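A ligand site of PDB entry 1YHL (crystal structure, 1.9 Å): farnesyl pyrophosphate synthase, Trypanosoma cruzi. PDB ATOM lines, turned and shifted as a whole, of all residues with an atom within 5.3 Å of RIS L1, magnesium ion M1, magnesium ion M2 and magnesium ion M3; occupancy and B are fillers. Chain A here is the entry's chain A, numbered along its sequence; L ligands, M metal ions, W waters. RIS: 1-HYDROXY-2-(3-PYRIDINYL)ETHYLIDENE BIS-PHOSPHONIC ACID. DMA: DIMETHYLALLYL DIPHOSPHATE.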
ATOM      1  N   TYR A  94      -5.942 -29.884  -4.864  1.00  0.00           N
ATOM      2  CA  TYR A  94      -7.099 -29.164  -4.224  1.00  0.00           C
ATOM      3  C   TYR A  94      -7.879 -28.273  -5.201  1.00  0.00           C
ATOM      4  O   TYR A  94      -9.108 -28.181  -5.135  1.00  0.00           O
ATOM      5  CB  TYR A  94      -6.628 -28.409  -2.925  1.00  0.00           C
ATOM      6  CG  TYR A  94      -6.688 -29.475  -1.782  1.00  0.00           C
ATOM      7  CD1 TYR A  94      -7.929 -30.063  -1.426  1.00  0.00           C
ATOM      8  CD2 TYR A  94      -5.578 -29.907  -1.167  1.00  0.00           C
ATOM      9  CE1 TYR A  94      -8.048 -31.061  -0.399  1.00  0.00           C
ATOM     10  CE2 TYR A  94      -5.606 -30.879  -0.151  1.00  0.00           C
ATOM     11  CZ  TYR A  94      -6.847 -31.508   0.223  1.00  0.00           C
ATOM     12  OH  TYR A  94      -6.926 -32.537   1.267  1.00  0.00           O
ATOM     13  N   LEU A  95      -7.164 -27.616  -6.120  1.00  0.00           N
ATOM     14  CA  LEU A  95      -7.847 -26.647  -7.028  1.00  0.00           C
ATOM     15  C   LEU A  95      -8.713 -27.403  -8.024  1.00  0.00           C
ATOM     16  O   LEU A  95      -9.799 -26.933  -8.388  1.00  0.00           O
ATOM     17  CB  LEU A  95      -6.817 -25.706  -7.733  1.00  0.00           C
ATOM     18  CG  LEU A  95      -5.983 -24.803  -6.802  1.00  0.00           C
ATOM     19  CD1 LEU A  95      -5.032 -23.861  -7.589  1.00  0.00           C
ATOM     20  CD2 LEU A  95      -6.952 -23.955  -5.826  1.00  0.00           C
ATOM     21  N   ASP A  98     -11.694 -28.437  -6.005  1.00  0.00           N
ATOM     22  CA  ASP A  98     -12.362 -27.189  -5.519  1.00  0.00           C
ATOM     23  C   ASP A  98     -13.217 -26.561  -6.701  1.00  0.00           C
ATOM     24  O   ASP A  98     -14.403 -26.160  -6.512  1.00  0.00           O
ATOM     25  CB  ASP A  98     -11.303 -26.170  -5.043  1.00  0.00           C
ATOM     26  CG  ASP A  98     -11.917 -24.835  -4.624  1.00  0.00           C
ATOM     27  OD1 ASP A  98     -12.457 -24.774  -3.500  1.00  0.00           O
ATOM     28  OD2 ASP A  98     -11.870 -23.854  -5.400  1.00  0.00           O
ATOM     29  N   ASP A  99     -12.634 -26.514  -7.903  1.00  0.00           N
ATOM     30  CA  ASP A  99     -13.352 -25.944  -9.030  1.00  0.00           C
ATOM     31  C   ASP A  99     -14.632 -26.685  -9.353  1.00  0.00           C
ATOM     32  O   ASP A  99     -15.632 -26.051  -9.694  1.00  0.00           O
ATOM     33  CB  ASP A  99     -12.481 -25.880 -10.271  1.00  0.00           C
ATOM     34  CG  ASP A  99     -11.516 -24.718 -10.226  1.00  0.00           C
ATOM     35  OD1 ASP A  99     -11.727 -23.754  -9.457  1.00  0.00           O
ATOM     36  OD2 ASP A  99     -10.504 -24.798 -10.943  1.00  0.00           O
ATOM     37  N   ASP A 102     -17.038 -25.833  -6.419  1.00  0.00           N
ATOM     38  CA  ASP A 102     -17.454 -24.447  -6.444  1.00  0.00           C
ATOM     39  C   ASP A 102     -18.268 -24.030  -7.676  1.00  0.00           C
ATOM     40  O   ASP A 102     -18.795 -22.901  -7.725  1.00  0.00           O
ATOM     41  CB  ASP A 102     -16.259 -23.518  -6.183  1.00  0.00           C
ATOM     42  CG  ASP A 102     -15.673 -23.660  -4.748  1.00  0.00           C
ATOM     43  OD1 ASP A 102     -16.312 -24.333  -3.938  1.00  0.00           O
ATOM     44  OD2 ASP A 102     -14.595 -23.078  -4.414  1.00  0.00           O
ATOM     45  N   SER A 104     -16.949 -23.534 -10.669  1.00  0.00           N
ATOM     46  CA  SER A 104     -16.212 -22.415 -11.241  1.00  0.00           C
ATOM     47  C   SER A 104     -15.985 -22.670 -12.725  1.00  0.00           C
ATOM     48  O   SER A 104     -16.015 -23.837 -13.175  1.00  0.00           O
ATOM     49  CB  SER A 104     -14.834 -22.337 -10.543  1.00  0.00           C
ATOM     50  OG  SER A 104     -14.987 -21.698  -9.285  1.00  0.00           O
ATOM     51  N   ARG A 107      -9.759 -20.954 -14.480  1.00  0.00           N
ATOM     52  CA  ARG A 107      -8.657 -21.073 -13.512  1.00  0.00           C
ATOM     53  C   ARG A 107      -7.410 -20.703 -14.325  1.00  0.00           C
ATOM     54  O   ARG A 107      -7.206 -21.275 -15.396  1.00  0.00           O
ATOM     55  CB  ARG A 107      -8.615 -22.551 -13.063  1.00  0.00           C
ATOM     56  CG  ARG A 107      -7.450 -23.093 -12.199  1.00  0.00           C
ATOM     57  CD  ARG A 107      -7.285 -22.553 -10.841  1.00  0.00           C
ATOM     58  NE  ARG A 107      -8.425 -22.906  -9.930  1.00  0.00           N
ATOM     59  CZ  ARG A 107      -8.682 -22.239  -8.811  1.00  0.00           C
ATOM     60  NH1 ARG A 107      -7.794 -21.292  -8.380  1.00  0.00           N
ATOM     61  NH2 ARG A 107      -9.708 -22.638  -8.044  1.00  0.00           N
ATOM     62  N   THR A 163      -6.342 -29.301   5.411  1.00  0.00           N
ATOM     63  CA  THR A 163      -6.930 -28.683   4.204  1.00  0.00           C
ATOM     64  C   THR A 163      -8.272 -29.339   3.841  1.00  0.00           C
ATOM     65  O   THR A 163      -9.279 -28.653   3.529  1.00  0.00           O
ATOM     66  CB  THR A 163      -5.929 -28.760   3.039  1.00  0.00           C
ATOM     67  OG1 THR A 163      -4.690 -28.107   3.416  1.00  0.00           O
ATOM     68  CG2 THR A 163      -6.506 -27.995   1.745  1.00  0.00           C
ATOM     69  N   GLN A 167     -11.790 -27.578   3.744  1.00  0.00           N
ATOM     70  CA  GLN A 167     -12.717 -27.598   2.601  1.00  0.00           C
ATOM     71  C   GLN A 167     -14.154 -28.057   2.994  1.00  0.00           C
ATOM     72  O   GLN A 167     -15.152 -27.552   2.408  1.00  0.00           O
ATOM     73  CB  GLN A 167     -12.163 -28.524   1.517  1.00  0.00           C
ATOM     74  CG  GLN A 167     -11.002 -27.862   0.740  1.00  0.00           C
ATOM     75  CD  GLN A 167     -11.507 -26.634  -0.049  1.00  0.00           C
ATOM     76  OE1 GLN A 167     -11.709 -25.504   0.495  1.00  0.00           O
ATOM     77  NE2 GLN A 167     -11.687 -26.842  -1.309  1.00  0.00           N
ATOM     78  N   ASP A 170     -15.712 -25.083   4.550  1.00  0.00           N
ATOM     79  CA  ASP A 170     -16.043 -24.092   3.495  1.00  0.00           C
ATOM     80  C   ASP A 170     -17.316 -24.448   2.685  1.00  0.00           C
ATOM     81  O   ASP A 170     -18.263 -23.624   2.539  1.00  0.00           O
ATOM     82  CB  ASP A 170     -14.833 -23.933   2.536  1.00  0.00           C
ATOM     83  CG  ASP A 170     -15.161 -23.049   1.357  1.00  0.00           C
ATOM     84  OD1 ASP A 170     -14.837 -21.882   1.433  1.00  0.00           O
ATOM     85  OD2 ASP A 170     -15.841 -23.517   0.414  1.00  0.00           O
ATOM     86  N   LYS A 207      -8.766 -24.399   5.568  1.00  0.00           N
ATOM     87  CA  LYS A 207      -8.798 -24.649   4.133  1.00  0.00           C
ATOM     88  C   LYS A 207      -7.631 -24.113   3.370  1.00  0.00           C
ATOM     89  O   LYS A 207      -7.345 -24.607   2.251  1.00  0.00           O
ATOM     90  CB  LYS A 207     -10.131 -24.189   3.498  1.00  0.00           C
ATOM     91  CG  LYS A 207     -10.240 -22.724   3.328  1.00  0.00           C
ATOM     92  CD  LYS A 207     -11.262 -22.352   2.237  1.00  0.00           C
ATOM     93  CE  LYS A 207     -11.371 -20.870   2.209  1.00  0.00           C
ATOM     94  NZ  LYS A 207     -12.402 -20.463   1.170  1.00  0.00           N
ATOM     95  N   THR A 208      -6.968 -23.065   3.917  1.00  0.00           N
ATOM     96  CA  THR A 208      -5.953 -22.414   3.105  1.00  0.00           C
ATOM     97  C   THR A 208      -4.604 -22.306   3.774  1.00  0.00           C
ATOM     98  O   THR A 208      -3.586 -22.511   3.151  1.00  0.00           O
ATOM     99  CB  THR A 208      -6.415 -20.969   2.636  1.00  0.00           C
ATOM    100  OG1 THR A 208      -7.413 -21.152   1.652  1.00  0.00           O
ATOM    101  CG2 THR A 208      -5.302 -20.145   1.985  1.00  0.00           C
ATOM    102  N   TYR A 211      -1.458 -25.280   3.794  1.00  0.00           N
ATOM    103  CA  TYR A 211      -0.691 -25.545   2.589  1.00  0.00           C
ATOM    104  C   TYR A 211      -0.106 -24.339   1.907  1.00  0.00           C
ATOM    105  O   TYR A 211       0.858 -24.498   1.213  1.00  0.00           O
ATOM    106  CB  TYR A 211      -1.454 -26.459   1.590  1.00  0.00           C
ATOM    107  CG  TYR A 211      -2.467 -25.748   0.706  1.00  0.00           C
ATOM    108  CD1 TYR A 211      -2.080 -25.227  -0.554  1.00  0.00           C
ATOM    109  CD2 TYR A 211      -3.771 -25.553   1.132  1.00  0.00           C
ATOM    110  CE1 TYR A 211      -2.974 -24.568  -1.393  1.00  0.00           C
ATOM    111  CE2 TYR A 211      -4.711 -24.913   0.274  1.00  0.00           C
ATOM    112  CZ  TYR A 211      -4.290 -24.407  -0.943  1.00  0.00           C
ATOM    113  OH  TYR A 211      -5.202 -23.769  -1.711  1.00  0.00           O
ATOM    114  N   GLN A 247      -6.041 -15.299   2.050  1.00  0.00           N
ATOM    115  CA  GLN A 247      -7.405 -15.677   1.704  1.00  0.00           C
ATOM    116  C   GLN A 247      -8.340 -14.477   1.719  1.00  0.00           C
ATOM    117  O   GLN A 247      -9.249 -14.345   0.893  1.00  0.00           O
ATOM    118  CB  GLN A 247      -7.867 -16.728   2.674  1.00  0.00           C
ATOM    119  CG  GLN A 247      -9.214 -17.347   2.328  1.00  0.00           C
ATOM    120  CD  GLN A 247      -9.230 -18.059   1.010  1.00  0.00           C
ATOM    121  OE1 GLN A 247      -8.409 -18.941   0.779  1.00  0.00           O
ATOM    122  NE2 GLN A 247     -10.201 -17.713   0.159  1.00  0.00           N
ATOM    123  N   ASP A 250      -7.962 -12.983  -1.560  1.00  0.00           N
ATOM    124  CA  ASP A 250      -8.691 -13.823  -2.548  1.00  0.00           C
ATOM    125  C   ASP A 250     -10.197 -13.526  -2.558  1.00  0.00           C
ATOM    126  O   ASP A 250     -10.811 -13.420  -3.612  1.00  0.00           O
ATOM    127  CB  ASP A 250      -8.504 -15.289  -2.130  1.00  0.00           C
ATOM    128  CG  ASP A 250      -8.949 -16.267  -3.207  1.00  0.00           C
ATOM    129  OD1 ASP A 250      -8.405 -16.229  -4.340  1.00  0.00           O
ATOM    130  OD2 ASP A 250      -9.856 -17.050  -2.904  1.00  0.00           O
ATOM    131  N   ASP A 251     -10.791 -13.383  -1.372  1.00  0.00           N
ATOM    132  CA  ASP A 251     -12.218 -13.113  -1.281  1.00  0.00           C
ATOM    133  C   ASP A 251     -12.571 -11.752  -1.912  1.00  0.00           C
ATOM    134  O   ASP A 251     -13.599 -11.632  -2.603  1.00  0.00           O
ATOM    135  CB  ASP A 251     -12.666 -13.156   0.190  1.00  0.00           C
ATOM    136  CG  ASP A 251     -12.588 -14.612   0.814  1.00  0.00           C
ATOM    137  OD1 ASP A 251     -12.264 -15.597   0.114  1.00  0.00           O
ATOM    138  OD2 ASP A 251     -12.883 -14.742   2.023  1.00  0.00           O
ATOM    139  N   ASP A 254     -12.353 -12.039  -5.722  1.00  0.00           N
ATOM    140  CA  ASP A 254     -13.457 -12.820  -6.282  1.00  0.00           C
ATOM    141  C   ASP A 254     -14.581 -11.902  -6.751  1.00  0.00           C
ATOM    142  O   ASP A 254     -15.132 -12.093  -7.821  1.00  0.00           O
ATOM    143  CB  ASP A 254     -14.035 -13.785  -5.251  1.00  0.00           C
ATOM    144  CG  ASP A 254     -14.984 -14.786  -5.872  1.00  0.00           C
ATOM    145  OD1 ASP A 254     -14.517 -15.809  -6.412  1.00  0.00           O
ATOM    146  OD2 ASP A 254     -16.212 -14.533  -5.895  1.00  0.00           O
ATOM    147  N   LYS A 264      -9.485 -15.848 -12.906  1.00  0.00           N
ATOM    148  CA  LYS A 264     -10.670 -16.614 -12.573  1.00  0.00           C
ATOM    149  C   LYS A 264     -11.959 -15.780 -12.596  1.00  0.00           C
ATOM    150  O   LYS A 264     -11.943 -14.545 -12.594  1.00  0.00           O
ATOM    151  CB  LYS A 264     -10.493 -17.381 -11.235  1.00  0.00           C
ATOM    152  CG  LYS A 264      -9.963 -16.591 -10.097  1.00  0.00           C
ATOM    153  CD  LYS A 264      -9.114 -17.504  -9.093  1.00  0.00           C
ATOM    154  CE  LYS A 264      -9.172 -16.867  -7.713  1.00  0.00           C
ATOM    155  NZ  LYS A 264      -8.223 -17.482  -6.705  1.00  0.00           N
ATOM    156  N   ASP A 268     -18.323 -16.541  -5.334  1.00  0.00           N
ATOM    157  CA  ASP A 268     -18.583 -16.606  -3.891  1.00  0.00           C
ATOM    158  C   ASP A 268     -19.984 -16.103  -3.585  1.00  0.00           C
ATOM    159  O   ASP A 268     -20.637 -16.664  -2.725  1.00  0.00           O
ATOM    160  CB  ASP A 268     -17.616 -15.742  -3.109  1.00  0.00           C
ATOM    161  CG  ASP A 268     -16.207 -16.337  -3.051  1.00  0.00           C
ATOM    162  OD1 ASP A 268     -15.989 -17.539  -3.369  1.00  0.00           O
ATOM    163  OD2 ASP A 268     -15.339 -15.589  -2.666  1.00  0.00           O
ATOM    164  N   LYS A 273     -20.952 -18.221  -0.184  1.00  0.00           N
ATOM    165  CA  LYS A 273     -19.800 -18.484   0.633  1.00  0.00           C
ATOM    166  C   LYS A 273     -19.751 -17.523   1.806  1.00  0.00           C
ATOM    167  O   LYS A 273     -20.185 -16.378   1.740  1.00  0.00           O
ATOM    168  CB  LYS A 273     -18.479 -18.404  -0.201  1.00  0.00           C
ATOM    169  CG  LYS A 273     -18.351 -19.629  -1.276  1.00  0.00           C
ATOM    170  CD  LYS A 273     -18.247 -20.906  -0.416  1.00  0.00           C
ATOM    171  CE  LYS A 273     -18.450 -22.229  -1.083  1.00  0.00           C
ATOM    172  NZ  LYS A 273     -17.858 -22.353  -2.407  1.00  0.00           N
HETATM  173  O12 RIS L   1     -11.317 -20.922  -6.062  1.00  0.00           O
HETATM  174  P9  RIS L   1     -10.262 -20.102  -5.384  1.00  0.00           P
HETATM  175  O11 RIS L   1     -10.562 -18.644  -5.408  1.00  0.00           O
HETATM  176  O10 RIS L   1      -8.953 -20.314  -6.209  1.00  0.00           O
HETATM  177  C8  RIS L   1      -9.959 -20.639  -3.673  1.00  0.00           C
HETATM  178  O13 RIS L   1      -8.994 -19.785  -3.091  1.00  0.00           O
HETATM  179  P14 RIS L   1     -11.502 -20.564  -2.693  1.00  0.00           P
HETATM  180  O16 RIS L   1     -12.106 -19.205  -2.807  1.00  0.00           O
HETATM  181  O15 RIS L   1     -12.234 -21.534  -3.516  1.00  0.00           O
HETATM  182  O17 RIS L   1     -11.457 -21.043  -1.276  1.00  0.00           O
HETATM  183  C7  RIS L   1      -9.349 -22.014  -3.815  1.00  0.00           C
HETATM  184  C2  RIS L   1      -8.988 -22.763  -2.654  1.00  0.00           C
HETATM  185  C1  RIS L   1      -9.060 -24.168  -2.746  1.00  0.00           C
HETATM  186  C6  RIS L   1      -8.783 -24.961  -1.614  1.00  0.00           C
HETATM  187  C5  RIS L   1      -8.420 -24.372  -0.406  1.00  0.00           C
HETATM  188  N4  RIS L   1      -8.274 -23.026  -0.304  1.00  0.00           N
HETATM  189  C3  RIS L   1      -8.565 -22.257  -1.393  1.00  0.00           C
HETATM  190  C1  DMA L   2      -2.098 -19.769  -5.116  1.00  0.00           C
HETATM  191  O1  DMA L   2      -1.214 -18.761  -5.741  1.00  0.00           O
HETATM  192  C2  DMA L   2      -3.645 -19.557  -5.158  1.00  0.00           C
HETATM  193  C3  DMA L   2      -4.730 -20.273  -4.687  1.00  0.00           C
HETATM  194  C4  DMA L   2      -6.113 -19.691  -4.934  1.00  0.00           C
HETATM  195  C5  DMA L   2      -4.679 -21.558  -3.878  1.00  0.00           C
HETATM  196  PA  DMA L   2       0.122 -18.798  -6.783  1.00  0.00           P
HETATM  197  O1A DMA L   2       1.247 -19.700  -6.416  1.00  0.00           O
HETATM  198  O2A DMA L   2       0.766 -17.409  -6.723  1.00  0.00           O
HETATM  199  O3A DMA L   2      -0.467 -18.820  -8.337  1.00  0.00           O
HETATM  200  PB  DMA L   2      -1.695 -19.862  -8.447  1.00  0.00           P
HETATM  201  O1B DMA L   2      -2.398 -19.850  -9.841  1.00  0.00           O
HETATM  202  O2B DMA L   2      -2.721 -19.339  -7.479  1.00  0.00           O
HETATM  203  O3B DMA L   2      -0.996 -21.086  -7.897  1.00  0.00           O
HETATM  204 MG    MG M   1     -12.950 -22.143  -5.397  1.00  0.00          MG
HETATM  205 MG    MG M   2     -11.733 -17.564  -3.876  1.00  0.00          MG
HETATM  206 MG    MG M   3     -13.548 -23.302  -2.610  1.00  0.00          MG
HETATM  207  O   HOH W   1      -6.775 -18.844  -1.802  1.00  0.00           O
HETATM  208  O   HOH W   2     -12.632 -16.324  -2.567  1.00  0.00           O
HETATM  209  O   HOH W   3     -14.915 -21.787  -1.721  1.00  0.00           O
HETATM  210  O   HOH W   4     -14.454 -19.256  -1.568  1.00  0.00           O
HETATM  211  O   HOH W   5     -12.347 -16.681  -7.660  1.00  0.00           O
HETATM  212  O   HOH W   6     -12.529 -23.482  -0.915  1.00  0.00           O
HETATM  213  O   HOH W   7     -12.122 -19.319  -8.127  1.00  0.00           O
HETATM  214  O   HOH W   8     -13.232 -22.699  -7.381  1.00  0.00           O
HETATM  215  O   HOH W   9     -11.517 -16.028  -5.221  1.00  0.00           O
HETATM  216  O   HOH W  10     -14.765 -24.874  -1.848  1.00  0.00           O
HETATM  217  O   HOH W  11     -14.212 -20.406  -5.632  1.00  0.00           O
HETATM  218  O   HOH W  12     -13.560 -17.808  -4.755  1.00  0.00           O
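The side-chain hydroxyl (OG1) of Thr 208 sits at hydrogen-bond distance from a nitrogen (N4) of RIS L1 (2.8 Å). OH of Tyr 211 lies within hydrogen-bond range of N4 of RIS L1, at 3.5 Å. The guanidinium group of Arg 107 lies within salt-bridge range of an oxygen (O10) of RIS L1, at 2.6 Å. An oxygen (O17) of RIS L1 lies within salt-bridge range of the side-chain amino group of Lys 207. The side-chain amino group of Lys 264 lies within salt-bridge range of an oxygen (O10) of RIS L1 (3.0 Å).
The side-chain carboxylate (OD1) of Asp 98 sits close to the side-chain amide nitrogen (NE2) of Gln 167. The side-chain hydroxyl (OG1) of Thr 208 sits at hydrogen-bond distance from the side-chain amide oxygen (OE1) of Gln 247 (2.6 Å). The side-chain amino group (NZ) of Lys 273 lies within salt-bridge range of the side-chain carboxylate (OD2) of Asp 170, at 3.7 Å. OD1 of Asp 99 lies within salt-bridge range of NH2 of Arg 107 (2.7 Å). OD1 of Asp 250 is in salt-bridge range of NZ of Lys 264 (2.7 Å). The side-chain carboxylate of Asp 102 lies within salt-bridge range of the side-chain amino group of Lys 273, at 2.9 Å. The side-chain amino group of Lys 207 lies within salt-bridge range of the side-chain carboxylate of Asp 170, 2.8 Å away. NE2 of Gln 247 sits close to OD2 of Asp 250 (3.2 Å).
Merely in contact with RIS L1: Leu 95, Gln 167 and Gln 247. Hydrophobic or aromatic side chains within 4 Å of RIS L1: Leu 95 and Tyr 211. Within 4 Å of RIS L1: Leu 95, Asp 98, Asp 102, Arg 107, Gln 167, Lys 207, Thr 208, Tyr 211, Gln 247, Asp 250 and Lys 264.
Two residues have an atom within 4 Å of magnesium ion M1: Asp 98 and Asp 102. The nearest printed residue that does not touch magnesium ion M1 is Arg 107 (4.2 Å).
One residue has an atom within 4 Å of magnesium ion M2: Asp 250.
OD2 of Asp 170 touches magnesium ion M3 (3.8 Å). Within 4 Å of magnesium ion M3: Asp 98, Asp 102 and Asp 170.
Magnesium ion M1 is bound by OD2 of Asp 98 (2.0 Å), water W8 (2.1 Å), O15 of RIS L1 (2.1 Å), OD2 of Asp 102 (2.1 Å), O12 of RIS L1 (2.1 Å) and water W11 (2.2 Å).
Magnesium ion M2 is bound by O16 of RIS L1, 2.0 Å away. Water W2 is bound to magnesium ion M2, 2.0 Å away. Magnesium ion M2 is bound by water W12 (2.0 Å). Water W9 is bound to magnesium ion M2 (2.1 Å). OD2 of Asp 250 binds magnesium ion M2 (2.2 Å). O11 of RIS L1 binds magnesium ion M2, at 2.2 Å. Magnesium ion M2 has six donor atoms within binding distance.
Water W6 is bound to magnesium ion M3. Magnesium ion M3 is bound by OD1 of Asp 98 (2.0 Å). Magnesium ion M3 is bound by the side-chain carboxylate (OD2) of Asp 102 (2.1 Å). Water W10 binds magnesium ion M3 (2.1 Å). Water W3 is bound to magnesium ion M3. Magnesium ion M3 is bound by O15 of RIS L1, at 2.4 Å. Magnesium ion M3 has six donor atoms within binding distance.
Water W8 bridges OD1 of Asp 99 and OG of Ser 104. Water W9 bridges O of Asp 250 (3.1 Å) and OD1 of Asp 254 (3.2 Å). Water W6 bridges the side-chain amide oxygen of Gln 167 (2.6 Å) and an oxygen (O17) of RIS L1 (2.7 Å). Water W10 lies within hydrogen-bond range of OD1 of Asp 102 and OD2 of Asp 170. Water W3 bridges OD2 of Asp 170 (2.9 Å) and NZ of Lys 273 (3.1 Å). Water W1 bridges O13 of RIS L1 (2.7 Å) and OE1 of Gln 247 (3.1 Å).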
